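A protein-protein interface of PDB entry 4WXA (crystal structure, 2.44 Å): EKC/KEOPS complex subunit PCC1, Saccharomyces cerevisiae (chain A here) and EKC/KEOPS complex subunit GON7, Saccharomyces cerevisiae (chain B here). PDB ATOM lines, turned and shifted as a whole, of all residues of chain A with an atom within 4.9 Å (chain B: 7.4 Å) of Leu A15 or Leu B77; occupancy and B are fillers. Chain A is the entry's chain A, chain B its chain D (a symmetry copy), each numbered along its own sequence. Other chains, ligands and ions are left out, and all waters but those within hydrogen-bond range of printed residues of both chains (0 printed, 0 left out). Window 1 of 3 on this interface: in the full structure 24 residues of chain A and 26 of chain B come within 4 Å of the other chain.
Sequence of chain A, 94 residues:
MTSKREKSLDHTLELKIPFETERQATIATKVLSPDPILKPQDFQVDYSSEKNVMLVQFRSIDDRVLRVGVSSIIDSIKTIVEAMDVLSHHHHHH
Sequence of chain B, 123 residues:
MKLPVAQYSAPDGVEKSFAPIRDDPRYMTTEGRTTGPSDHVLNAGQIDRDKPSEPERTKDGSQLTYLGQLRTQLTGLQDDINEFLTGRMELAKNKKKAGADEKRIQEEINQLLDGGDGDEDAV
The backbone carbonyl oxygen (O) of Gln B7 lies within hydrogen-bond range of the backbone NH (N) of Glu A14 (2.8 Å).
The backbone NH of Lys A16 lies within hydrogen-bond range of the backbone carbonyl oxygen of Val B5, 2.8 Å away.
The backbone carbonyl oxygen (O) of Leu A13 is in hydrogen-bond range of the backbone NH (N) of Phe A58, 2.8 Å away.
The backbone carbonyl oxygen (O) of Val A56 lies within hydrogen-bond range of the backbone NH (N) of Leu A15, at 2.8 Å.
The backbone NH (N) of Phe B18 lies within hydrogen-bond range of the backbone carbonyl oxygen (O) of Ala B6 (2.8 Å).
The side-chain amide oxygen of Gln B7 is in hydrogen-bond range of the side-chain hydroxyl of Ser B17 (2.8 Å).
The backbone carbonyl oxygen (O) of Gln B78 is in hydrogen-bond range of the side-chain amide nitrogen (ND2) of Asn B82, at 3.3 Å.
Among the printed residues, merely in contact across the chains: Glu A14 with Ala B6, Leu A13 with Gln B7, Lys A16 with Pro B4, Leu A15 with Val B5, Leu A15 with Leu B77, Ile A74 with Gln B78, Glu A14 with Val B5, Ile A77 with Leu B74 and Leu A13 with Ile B81.
Of the printed residues of chain B, Glu A14 touches Val B5 (3.9 Å), Ala B6 (3.0 Å) and Gln B7 (2.8 Å).
Leu A15 touches two residues of chain B.
Met A54 touches none of the printed residues of chain B.
Printed residues of chain B within 4 Å of Ile A77: Leu B74.
The nearest residue of chain B that does not touch Leu A15 is Ala B6 (4.2 Å).
Hydrophobic or aromatic side chains of chain B within 4 Å of the printed part of chain A: Pro B4, Val B5, Ala B6, Leu B74, Leu B77 and Ile B81.
Hydrophobic or aromatic side chains of chain A that line the printed part of chain B: Leu A13, Leu A15, Ile A74 and Ile A77.
Among the printed residues, 11 pairs touch across the chains.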
ATOM      1  N   LEU A  13      19.157   7.318  -1.730  1.00  0.00           N
ATOM      2  CA  LEU A  13      19.223   8.340  -0.749  1.00  0.00           C
ATOM      3  C   LEU A  13      18.085   8.172   0.281  1.00  0.00           C
ATOM      4  O   LEU A  13      16.963   7.814  -0.057  1.00  0.00           O
ATOM      5  CB  LEU A  13      19.086   9.652  -1.453  1.00  0.00           C
ATOM      6  CG  LEU A  13      19.328  10.899  -0.596  1.00  0.00           C
ATOM      7  CD1 LEU A  13      19.848  11.929  -1.505  1.00  0.00           C
ATOM      8  CD2 LEU A  13      18.069  11.455  -0.016  1.00  0.00           C
ATOM      9  N   GLU A  14      18.382   8.407   1.536  1.00  0.00           N
ATOM     10  CA  GLU A  14      17.340   8.363   2.571  1.00  0.00           C
ATOM     11  C   GLU A  14      17.332   9.665   3.302  1.00  0.00           C
ATOM     12  O   GLU A  14      18.336  10.202   3.783  1.00  0.00           O
ATOM     13  CB  GLU A  14      17.485   7.185   3.506  1.00  0.00           C
ATOM     14  CG  GLU A  14      16.660   7.372   4.768  1.00  0.00           C
ATOM     15  CD  GLU A  14      16.141   6.081   5.368  1.00  0.00           C
ATOM     16  OE1 GLU A  14      16.953   5.297   5.901  1.00  0.00           O
ATOM     17  OE2 GLU A  14      14.912   5.866   5.354  1.00  0.00           O
ATOM     18  N   LEU A  15      16.151  10.183   3.372  1.00  0.00           N
ATOM     19  CA  LEU A  15      15.920  11.419   4.018  1.00  0.00           C
ATOM     20  C   LEU A  15      15.118  11.215   5.333  1.00  0.00           C
ATOM     21  O   LEU A  15      14.110  10.498   5.343  1.00  0.00           O
ATOM     22  CB  LEU A  15      15.148  12.202   3.031  1.00  0.00           C
ATOM     23  CG  LEU A  15      14.745  13.598   3.441  1.00  0.00           C
ATOM     24  CD1 LEU A  15      15.939  14.506   3.709  1.00  0.00           C
ATOM     25  CD2 LEU A  15      13.946  14.186   2.277  1.00  0.00           C
ATOM     26  N   LYS A  16      15.587  11.761   6.451  1.00  0.00           N
ATOM     27  CA  LYS A  16      14.824  11.618   7.764  1.00  0.00           C
ATOM     28  C   LYS A  16      14.397  12.974   8.297  1.00  0.00           C
ATOM     29  O   LYS A  16      15.228  13.871   8.446  1.00  0.00           O
ATOM     30  CB  LYS A  16      15.650  10.931   8.814  1.00  0.00           C
ATOM     31  CG  LYS A  16      16.471   9.746   8.334  1.00  0.00           C
ATOM     32  CD  LYS A  16      17.084   9.091   9.542  1.00  0.00           C
ATOM     33  CE  LYS A  16      17.639   7.720   9.273  1.00  0.00           C
ATOM     34  NZ  LYS A  16      18.888   7.730   8.471  1.00  0.00           N
ATOM     35  N   ILE A  17      13.107  13.140   8.559  1.00  0.00           N
ATOM     36  CA  ILE A  17      12.572  14.449   8.873  1.00  0.00           C
ATOM     37  C   ILE A  17      11.842  14.438  10.225  1.00  0.00           C
ATOM     38  O   ILE A  17      10.753  13.927  10.327  1.00  0.00           O
ATOM     39  CB  ILE A  17      11.615  14.890   7.768  1.00  0.00           C
ATOM     40  CG1 ILE A  17      12.400  15.057   6.451  1.00  0.00           C
ATOM     41  CG2 ILE A  17      10.938  16.218   8.052  1.00  0.00           C
ATOM     42  CD1 ILE A  17      11.621  14.400   5.352  1.00  0.00           C
ATOM     43  N   MET A  54       9.577  11.248   9.925  1.00  0.00           N
ATOM     44  CA  MET A  54       9.207  10.782   8.585  1.00  0.00           C
ATOM     45  C   MET A  54      10.451  10.248   7.833  1.00  0.00           C
ATOM     46  O   MET A  54      11.484  10.886   7.815  1.00  0.00           O
ATOM     47  CB  MET A  54       8.546  11.893   7.813  1.00  0.00           C
ATOM     48  CG  MET A  54       8.061  11.440   6.432  1.00  0.00           C
ATOM     49  SD  MET A  54       7.679  12.893   5.392  1.00  0.00           S
ATOM     50  CE  MET A  54       6.342  12.237   4.453  1.00  0.00           C
ATOM     51  N   LEU A  55      10.330   9.057   7.242  1.00  0.00           N
ATOM     52  CA  LEU A  55      11.399   8.396   6.577  1.00  0.00           C
ATOM     53  C   LEU A  55      11.032   8.329   5.071  1.00  0.00           C
ATOM     54  O   LEU A  55       9.941   7.857   4.727  1.00  0.00           O
ATOM     55  CB  LEU A  55      11.593   7.052   7.216  1.00  0.00           C
ATOM     56  CG  LEU A  55      11.747   7.013   8.713  1.00  0.00           C
ATOM     57  CD1 LEU A  55      11.754   5.619   9.305  1.00  0.00           C
ATOM     58  CD2 LEU A  55      13.050   7.673   9.161  1.00  0.00           C
ATOM     59  N   VAL A  56      11.905   8.880   4.182  1.00  0.00           N
ATOM     60  CA  VAL A  56      11.686   8.795   2.739  1.00  0.00           C
ATOM     61  C   VAL A  56      12.951   8.198   2.067  1.00  0.00           C
ATOM     62  O   VAL A  56      14.047   8.776   2.084  1.00  0.00           O
ATOM     63  CB  VAL A  56      11.506  10.181   2.132  1.00  0.00           C
ATOM     64  CG1 VAL A  56      11.036  10.094   0.682  1.00  0.00           C
ATOM     65  CG2 VAL A  56      10.459  10.957   2.834  1.00  0.00           C
ATOM     66  N   PHE A  58      14.593   7.007  -1.368  1.00  0.00           N
ATOM     67  CA  PHE A  58      14.702   7.006  -2.845  1.00  0.00           C
ATOM     68  C   PHE A  58      15.684   5.948  -3.343  1.00  0.00           C
ATOM     69  O   PHE A  58      16.683   5.662  -2.685  1.00  0.00           O
ATOM     70  CB  PHE A  58      15.209   8.358  -3.307  1.00  0.00           C
ATOM     71  CG  PHE A  58      14.468   9.515  -2.728  1.00  0.00           C
ATOM     72  CD1 PHE A  58      14.793  10.004  -1.488  1.00  0.00           C
ATOM     73  CD2 PHE A  58      13.442  10.127  -3.427  1.00  0.00           C
ATOM     74  CE1 PHE A  58      14.106  11.096  -0.928  1.00  0.00           C
ATOM     75  CE2 PHE A  58      12.755  11.199  -2.892  1.00  0.00           C
ATOM     76  CZ  PHE A  58      13.091  11.686  -1.619  1.00  0.00           C
ATOM     77  N   ILE A  74      11.098  16.877  -1.957  1.00  0.00           N
ATOM     78  CA  ILE A  74      11.432  17.798  -0.899  1.00  0.00           C
ATOM     79  C   ILE A  74      10.577  19.060  -0.975  1.00  0.00           C
ATOM     80  O   ILE A  74      10.203  19.611   0.058  1.00  0.00           O
ATOM     81  CB  ILE A  74      12.906  18.130  -0.890  1.00  0.00           C
ATOM     82  CG1 ILE A  74      13.685  16.879  -0.462  1.00  0.00           C
ATOM     83  CG2 ILE A  74      13.195  19.263   0.078  1.00  0.00           C
ATOM     84  CD1 ILE A  74      15.217  17.060  -0.391  1.00  0.00           C
ATOM     85  N   ILE A  77       7.273  18.303   0.692  1.00  0.00           N
ATOM     86  CA  ILE A  77       7.432  18.154   2.107  1.00  0.00           C
ATOM     87  C   ILE A  77       7.494  19.525   2.782  1.00  0.00           C
ATOM     88  O   ILE A  77       6.817  19.765   3.790  1.00  0.00           O
ATOM     89  CB  ILE A  77       8.674  17.358   2.435  1.00  0.00           C
ATOM     90  CG1 ILE A  77       8.527  15.907   1.974  1.00  0.00           C
ATOM     91  CG2 ILE A  77       8.917  17.421   3.925  1.00  0.00           C
ATOM     92  CD1 ILE A  77       9.866  15.124   2.063  1.00  0.00           C
ATOM     93  N   LEU B   3      17.974  17.327  13.912  1.00  0.00           N
ATOM     94  CA  LEU B   3      17.877  17.981  12.627  1.00  0.00           C
ATOM     95  C   LEU B   3      17.400  17.004  11.561  1.00  0.00           C
ATOM     96  O   LEU B   3      17.554  15.798  11.690  1.00  0.00           O
ATOM     97  CB  LEU B   3      19.234  18.495  12.216  1.00  0.00           C
ATOM     98  CG  LEU B   3      20.067  19.267  13.237  1.00  0.00           C
ATOM     99  CD1 LEU B   3      21.531  19.304  12.793  1.00  0.00           C
ATOM    100  CD2 LEU B   3      19.496  20.665  13.364  1.00  0.00           C
ATOM    101  N   PRO B   4      16.854  17.531  10.480  1.00  0.00           N
ATOM    102  CA  PRO B   4      16.666  16.642   9.377  1.00  0.00           C
ATOM    103  C   PRO B   4      18.006  16.165   8.839  1.00  0.00           C
ATOM    104  O   PRO B   4      18.904  16.949   8.841  1.00  0.00           O
ATOM    105  CB  PRO B   4      15.952  17.512   8.350  1.00  0.00           C
ATOM    106  CG  PRO B   4      16.357  18.890   8.673  1.00  0.00           C
ATOM    107  CD  PRO B   4      16.548  18.925  10.151  1.00  0.00           C
ATOM    108  N   VAL B   5      18.113  14.909   8.373  1.00  0.00           N
ATOM    109  CA  VAL B   5      19.350  14.414   7.771  1.00  0.00           C
ATOM    110  C   VAL B   5      19.107  13.590   6.497  1.00  0.00           C
ATOM    111  O   VAL B   5      17.982  13.235   6.163  1.00  0.00           O
ATOM    112  CB  VAL B   5      20.157  13.515   8.752  1.00  0.00           C
ATOM    113  CG1 VAL B   5      20.565  14.293  10.015  1.00  0.00           C
ATOM    114  CG2 VAL B   5      19.361  12.246   9.064  1.00  0.00           C
ATOM    115  N   ALA B   6      20.197  13.292   5.807  1.00  0.00           N
ATOM    116  CA  ALA B   6      20.144  12.438   4.667  1.00  0.00           C
ATOM    117  C   ALA B   6      21.404  11.621   4.501  1.00  0.00           C
ATOM    118  O   ALA B   6      22.483  12.063   4.875  1.00  0.00           O
ATOM    119  CB  ALA B   6      19.921  13.274   3.459  1.00  0.00           C
ATOM    120  N   GLN B   7      21.250  10.417   3.954  1.00  0.00           N
ATOM    121  CA  GLN B   7      22.383   9.565   3.657  1.00  0.00           C
ATOM    122  C   GLN B   7      22.244   9.072   2.163  1.00  0.00           C
ATOM    123  O   GLN B   7      21.162   8.660   1.722  1.00  0.00           O
ATOM    124  CB  GLN B   7      22.384   8.423   4.659  1.00  0.00           C
ATOM    125  CG  GLN B   7      23.400   7.310   4.466  1.00  0.00           C
ATOM    126  CD  GLN B   7      24.817   7.739   4.751  1.00  0.00           C
ATOM    127  OE1 GLN B   7      25.090   8.509   5.692  1.00  0.00           O
ATOM    128  NE2 GLN B   7      25.734   7.240   3.950  1.00  0.00           N
ATOM    129  N   SER B  17      27.029  11.486   3.850  1.00  0.00           N
ATOM    130  CA  SER B  17      26.086  12.061   4.836  1.00  0.00           C
ATOM    131  C   SER B  17      25.845  13.536   4.666  1.00  0.00           C
ATOM    132  O   SER B  17      26.783  14.315   4.432  1.00  0.00           O
ATOM    133  CB  SER B  17      26.618  11.882   6.247  1.00  0.00           C
ATOM    134  OG  SER B  17      26.809  10.519   6.465  1.00  0.00           O
ATOM    135  N   PHE B  18      24.595  13.925   4.836  1.00  0.00           N
ATOM    136  CA  PHE B  18      24.206  15.315   4.881  1.00  0.00           C
ATOM    137  C   PHE B  18      23.605  15.711   6.226  1.00  0.00           C
ATOM    138  O   PHE B  18      22.772  15.004   6.804  1.00  0.00           O
ATOM    139  CB  PHE B  18      23.137  15.554   3.852  1.00  0.00           C
ATOM    140  CG  PHE B  18      23.535  15.220   2.447  1.00  0.00           C
ATOM    141  CD1 PHE B  18      23.320  13.971   1.937  1.00  0.00           C
ATOM    142  CD2 PHE B  18      24.061  16.182   1.619  1.00  0.00           C
ATOM    143  CE1 PHE B  18      23.671  13.662   0.628  1.00  0.00           C
ATOM    144  CE2 PHE B  18      24.381  15.894   0.316  1.00  0.00           C
ATOM    145  CZ  PHE B  18      24.191  14.628  -0.191  1.00  0.00           C
ATOM    146  N   ALA B  19      24.015  16.857   6.711  1.00  0.00           N
ATOM    147  CA  ALA B  19      23.427  17.481   7.884  1.00  0.00           C
ATOM    148  C   ALA B  19      23.582  18.950   7.634  1.00  0.00           C
ATOM    149  O   ALA B  19      24.644  19.396   7.222  1.00  0.00           O
ATOM    150  CB  ALA B  19      24.171  17.078   9.140  1.00  0.00           C
ATOM    151  N   PRO B  20      22.544  19.718   7.882  1.00  0.00           N
ATOM    152  CA  PRO B  20      22.621  21.188   7.776  1.00  0.00           C
ATOM    153  C   PRO B  20      23.639  21.840   8.729  1.00  0.00           C
ATOM    154  O   PRO B  20      23.707  21.472   9.911  1.00  0.00           O
ATOM    155  CB  PRO B  20      21.208  21.633   8.153  1.00  0.00           C
ATOM    156  CG  PRO B  20      20.694  20.544   9.044  1.00  0.00           C
ATOM    157  CD  PRO B  20      21.334  19.265   8.585  1.00  0.00           C
ATOM    158  N   ARG B  71      11.756  23.999   8.169  1.00  0.00           N
ATOM    159  CA  ARG B  71      11.597  24.259   6.750  1.00  0.00           C
ATOM    160  C   ARG B  71      12.861  24.917   6.126  1.00  0.00           C
ATOM    161  O   ARG B  71      13.192  24.623   4.984  1.00  0.00           O
ATOM    162  CB  ARG B  71      10.368  25.132   6.494  1.00  0.00           C
ATOM    163  CG  ARG B  71      10.085  25.454   5.033  1.00  0.00           C
ATOM    164  CD  ARG B  71       8.637  25.889   4.788  1.00  0.00           C
ATOM    165  NE  ARG B  71       8.386  27.300   5.116  1.00  0.00           N
ATOM    166  N   THR B  72      13.549  25.786   6.851  1.00  0.00           N
ATOM    167  CA  THR B  72      14.737  26.374   6.297  1.00  0.00           C
ATOM    168  C   THR B  72      15.791  25.301   6.253  1.00  0.00           C
ATOM    169  O   THR B  72      16.475  25.137   5.226  1.00  0.00           O
ATOM    170  CB  THR B  72      15.216  27.644   7.014  1.00  0.00           C
ATOM    171  OG1 THR B  72      15.355  27.421   8.418  1.00  0.00           O
ATOM    172  CG2 THR B  72      14.224  28.768   6.773  1.00  0.00           C
ATOM    173  N   GLN B  73      15.880  24.503   7.313  1.00  0.00           N
ATOM    174  CA  GLN B  73      16.860  23.438   7.306  1.00  0.00           C
ATOM    175  C   GLN B  73      16.638  22.517   6.099  1.00  0.00           C
ATOM    176  O   GLN B  73      17.609  22.034   5.486  1.00  0.00           O
ATOM    177  CB  GLN B  73      16.815  22.637   8.581  1.00  0.00           C
ATOM    178  CG  GLN B  73      17.405  23.325   9.779  1.00  0.00           C
ATOM    179  CD  GLN B  73      16.875  22.751  11.079  1.00  0.00           C
ATOM    180  OE1 GLN B  73      15.843  22.066  11.108  1.00  0.00           O
ATOM    181  NE2 GLN B  73      17.578  23.016  12.160  1.00  0.00           N
ATOM    182  N   LEU B  74      15.382  22.259   5.749  1.00  0.00           N
ATOM    183  CA  LEU B  74      15.136  21.375   4.620  1.00  0.00           C
ATOM    184  C   LEU B  74      15.546  22.041   3.348  1.00  0.00           C
ATOM    185  O   LEU B  74      15.919  21.382   2.409  1.00  0.00           O
ATOM    186  CB  LEU B  74      13.667  21.042   4.479  1.00  0.00           C
ATOM    187  CG  LEU B  74      13.100  20.043   5.457  1.00  0.00           C
ATOM    188  CD1 LEU B  74      11.593  19.936   5.237  1.00  0.00           C
ATOM    189  CD2 LEU B  74      13.811  18.714   5.291  1.00  0.00           C
ATOM    190  N   THR B  75      15.416  23.354   3.297  1.00  0.00           N
ATOM    191  CA  THR B  75      15.835  24.074   2.103  1.00  0.00           C
ATOM    192  C   THR B  75      17.372  23.985   1.908  1.00  0.00           C
ATOM    193  O   THR B  75      17.858  23.827   0.805  1.00  0.00           O
ATOM    194  CB  THR B  75      15.360  25.536   2.142  1.00  0.00           C
ATOM    195  OG1 THR B  75      13.928  25.567   2.002  1.00  0.00           O
ATOM    196  CG2 THR B  75      16.005  26.332   0.991  1.00  0.00           C
ATOM    197  N   GLY B  76      18.100  24.048   3.009  1.00  0.00           N
ATOM    198  CA  GLY B  76      19.537  23.906   3.012  1.00  0.00           C
ATOM    199  C   GLY B  76      19.993  22.506   2.679  1.00  0.00           C
ATOM    200  O   GLY B  76      21.025  22.308   2.021  1.00  0.00           O
ATOM    201  N   LEU B  77      19.229  21.521   3.124  1.00  0.00           N
ATOM    202  CA  LEU B  77      19.590  20.137   2.840  1.00  0.00           C
ATOM    203  C   LEU B  77      19.413  19.871   1.332  1.00  0.00           C
ATOM    204  O   LEU B  77      20.197  19.197   0.705  1.00  0.00           O
ATOM    205  CB  LEU B  77      18.707  19.210   3.689  1.00  0.00           C
ATOM    206  CG  LEU B  77      19.147  17.796   4.032  1.00  0.00           C
ATOM    207  CD1 LEU B  77      20.520  17.852   4.706  1.00  0.00           C
ATOM    208  CD2 LEU B  77      18.103  17.135   4.937  1.00  0.00           C
ATOM    209  N   GLN B  78      18.333  20.402   0.793  1.00  0.00           N
ATOM    210  CA  GLN B  78      17.970  20.276  -0.595  1.00  0.00           C
ATOM    211  C   GLN B  78      19.028  20.885  -1.495  1.00  0.00           C
ATOM    212  O   GLN B  78      19.227  20.434  -2.606  1.00  0.00           O
ATOM    213  CB  GLN B  78      16.657  21.029  -0.821  1.00  0.00           C
ATOM    214  CG  GLN B  78      16.102  20.993  -2.224  1.00  0.00           C
ATOM    215  CD  GLN B  78      14.796  21.742  -2.327  1.00  0.00           C
ATOM    216  OE1 GLN B  78      14.613  22.761  -1.684  1.00  0.00           O
ATOM    217  NE2 GLN B  78      13.880  21.240  -3.131  1.00  0.00           N
ATOM    218  N   ASP B  79      19.677  21.931  -1.025  1.00  0.00           N
ATOM    219  CA  ASP B  79      20.712  22.557  -1.803  1.00  0.00           C
ATOM    220  C   ASP B  79      21.964  21.695  -1.742  1.00  0.00           C
ATOM    221  O   ASP B  79      22.582  21.433  -2.790  1.00  0.00           O
ATOM    222  CB  ASP B  79      20.973  23.984  -1.300  1.00  0.00           C
ATOM    223  CG  ASP B  79      19.815  24.944  -1.611  1.00  0.00           C
ATOM    224  OD1 ASP B  79      18.890  24.540  -2.351  1.00  0.00           O
ATOM    225  OD2 ASP B  79      19.828  26.099  -1.129  1.00  0.00           O
ATOM    226  N   ASP B  80      22.326  21.236  -0.536  1.00  0.00           N
ATOM    227  CA  ASP B  80      23.441  20.285  -0.376  1.00  0.00           C
ATOM    228  C   ASP B  80      23.284  19.091  -1.351  1.00  0.00           C
ATOM    229  O   ASP B  80      24.189  18.754  -2.105  1.00  0.00           O
ATOM    230  CB  ASP B  80      23.556  19.735   1.053  1.00  0.00           C
ATOM    231  CG  ASP B  80      23.886  20.769   2.105  1.00  0.00           C
ATOM    232  OD1 ASP B  80      24.357  21.903   1.796  1.00  0.00           O
ATOM    233  OD2 ASP B  80      23.667  20.391   3.294  1.00  0.00           O
ATOM    234  N   ILE B  81      22.135  18.461  -1.346  1.00  0.00           N
ATOM    235  CA  ILE B  81      21.904  17.278  -2.162  1.00  0.00           C
ATOM    236  C   ILE B  81      22.084  17.652  -3.631  1.00  0.00           C
ATOM    237  O   ILE B  81      22.749  16.949  -4.374  1.00  0.00           O
ATOM    238  CB  ILE B  81      20.512  16.710  -1.894  1.00  0.00           C
ATOM    239  CG1 ILE B  81      20.482  16.043  -0.518  1.00  0.00           C
ATOM    240  CG2 ILE B  81      20.094  15.606  -2.849  1.00  0.00           C
ATOM    241  CD1 ILE B  81      19.102  15.961   0.114  1.00  0.00           C
ATOM    242  N   ASN B  82      21.501  18.771  -4.039  1.00  0.00           N
ATOM    243  CA  ASN B  82      21.546  19.199  -5.421  1.00  0.00           C
ATOM    244  C   ASN B  82      22.991  19.537  -5.792  1.00  0.00           C
ATOM    245  O   ASN B  82      23.510  19.088  -6.814  1.00  0.00           O
ATOM    246  CB  ASN B  82      20.587  20.382  -5.667  1.00  0.00           C
ATOM    247  CG  ASN B  82      19.153  19.938  -6.072  1.00  0.00           C
ATOM    248  OD1 ASN B  82      18.927  18.879  -6.669  1.00  0.00           O
ATOM    249  ND2 ASN B  82      18.178  20.764  -5.737  1.00  0.00           N
ATOM    250  N   GLU B  83      23.656  20.281  -4.935  1.00  0.00           N
ATOM    251  CA  GLU B  83      25.063  20.551  -5.152  1.00  0.00           C
ATOM    252  C   GLU B  83      25.875  19.238  -5.297  1.00  0.00           C
ATOM    253  O   GLU B  83      26.633  19.069  -6.220  1.00  0.00           O
ATOM    254  CB  GLU B  83      25.603  21.444  -4.025  1.00  0.00           C
ATOM    255  CG  GLU B  83      27.068  21.866  -4.158  1.00  0.00           C
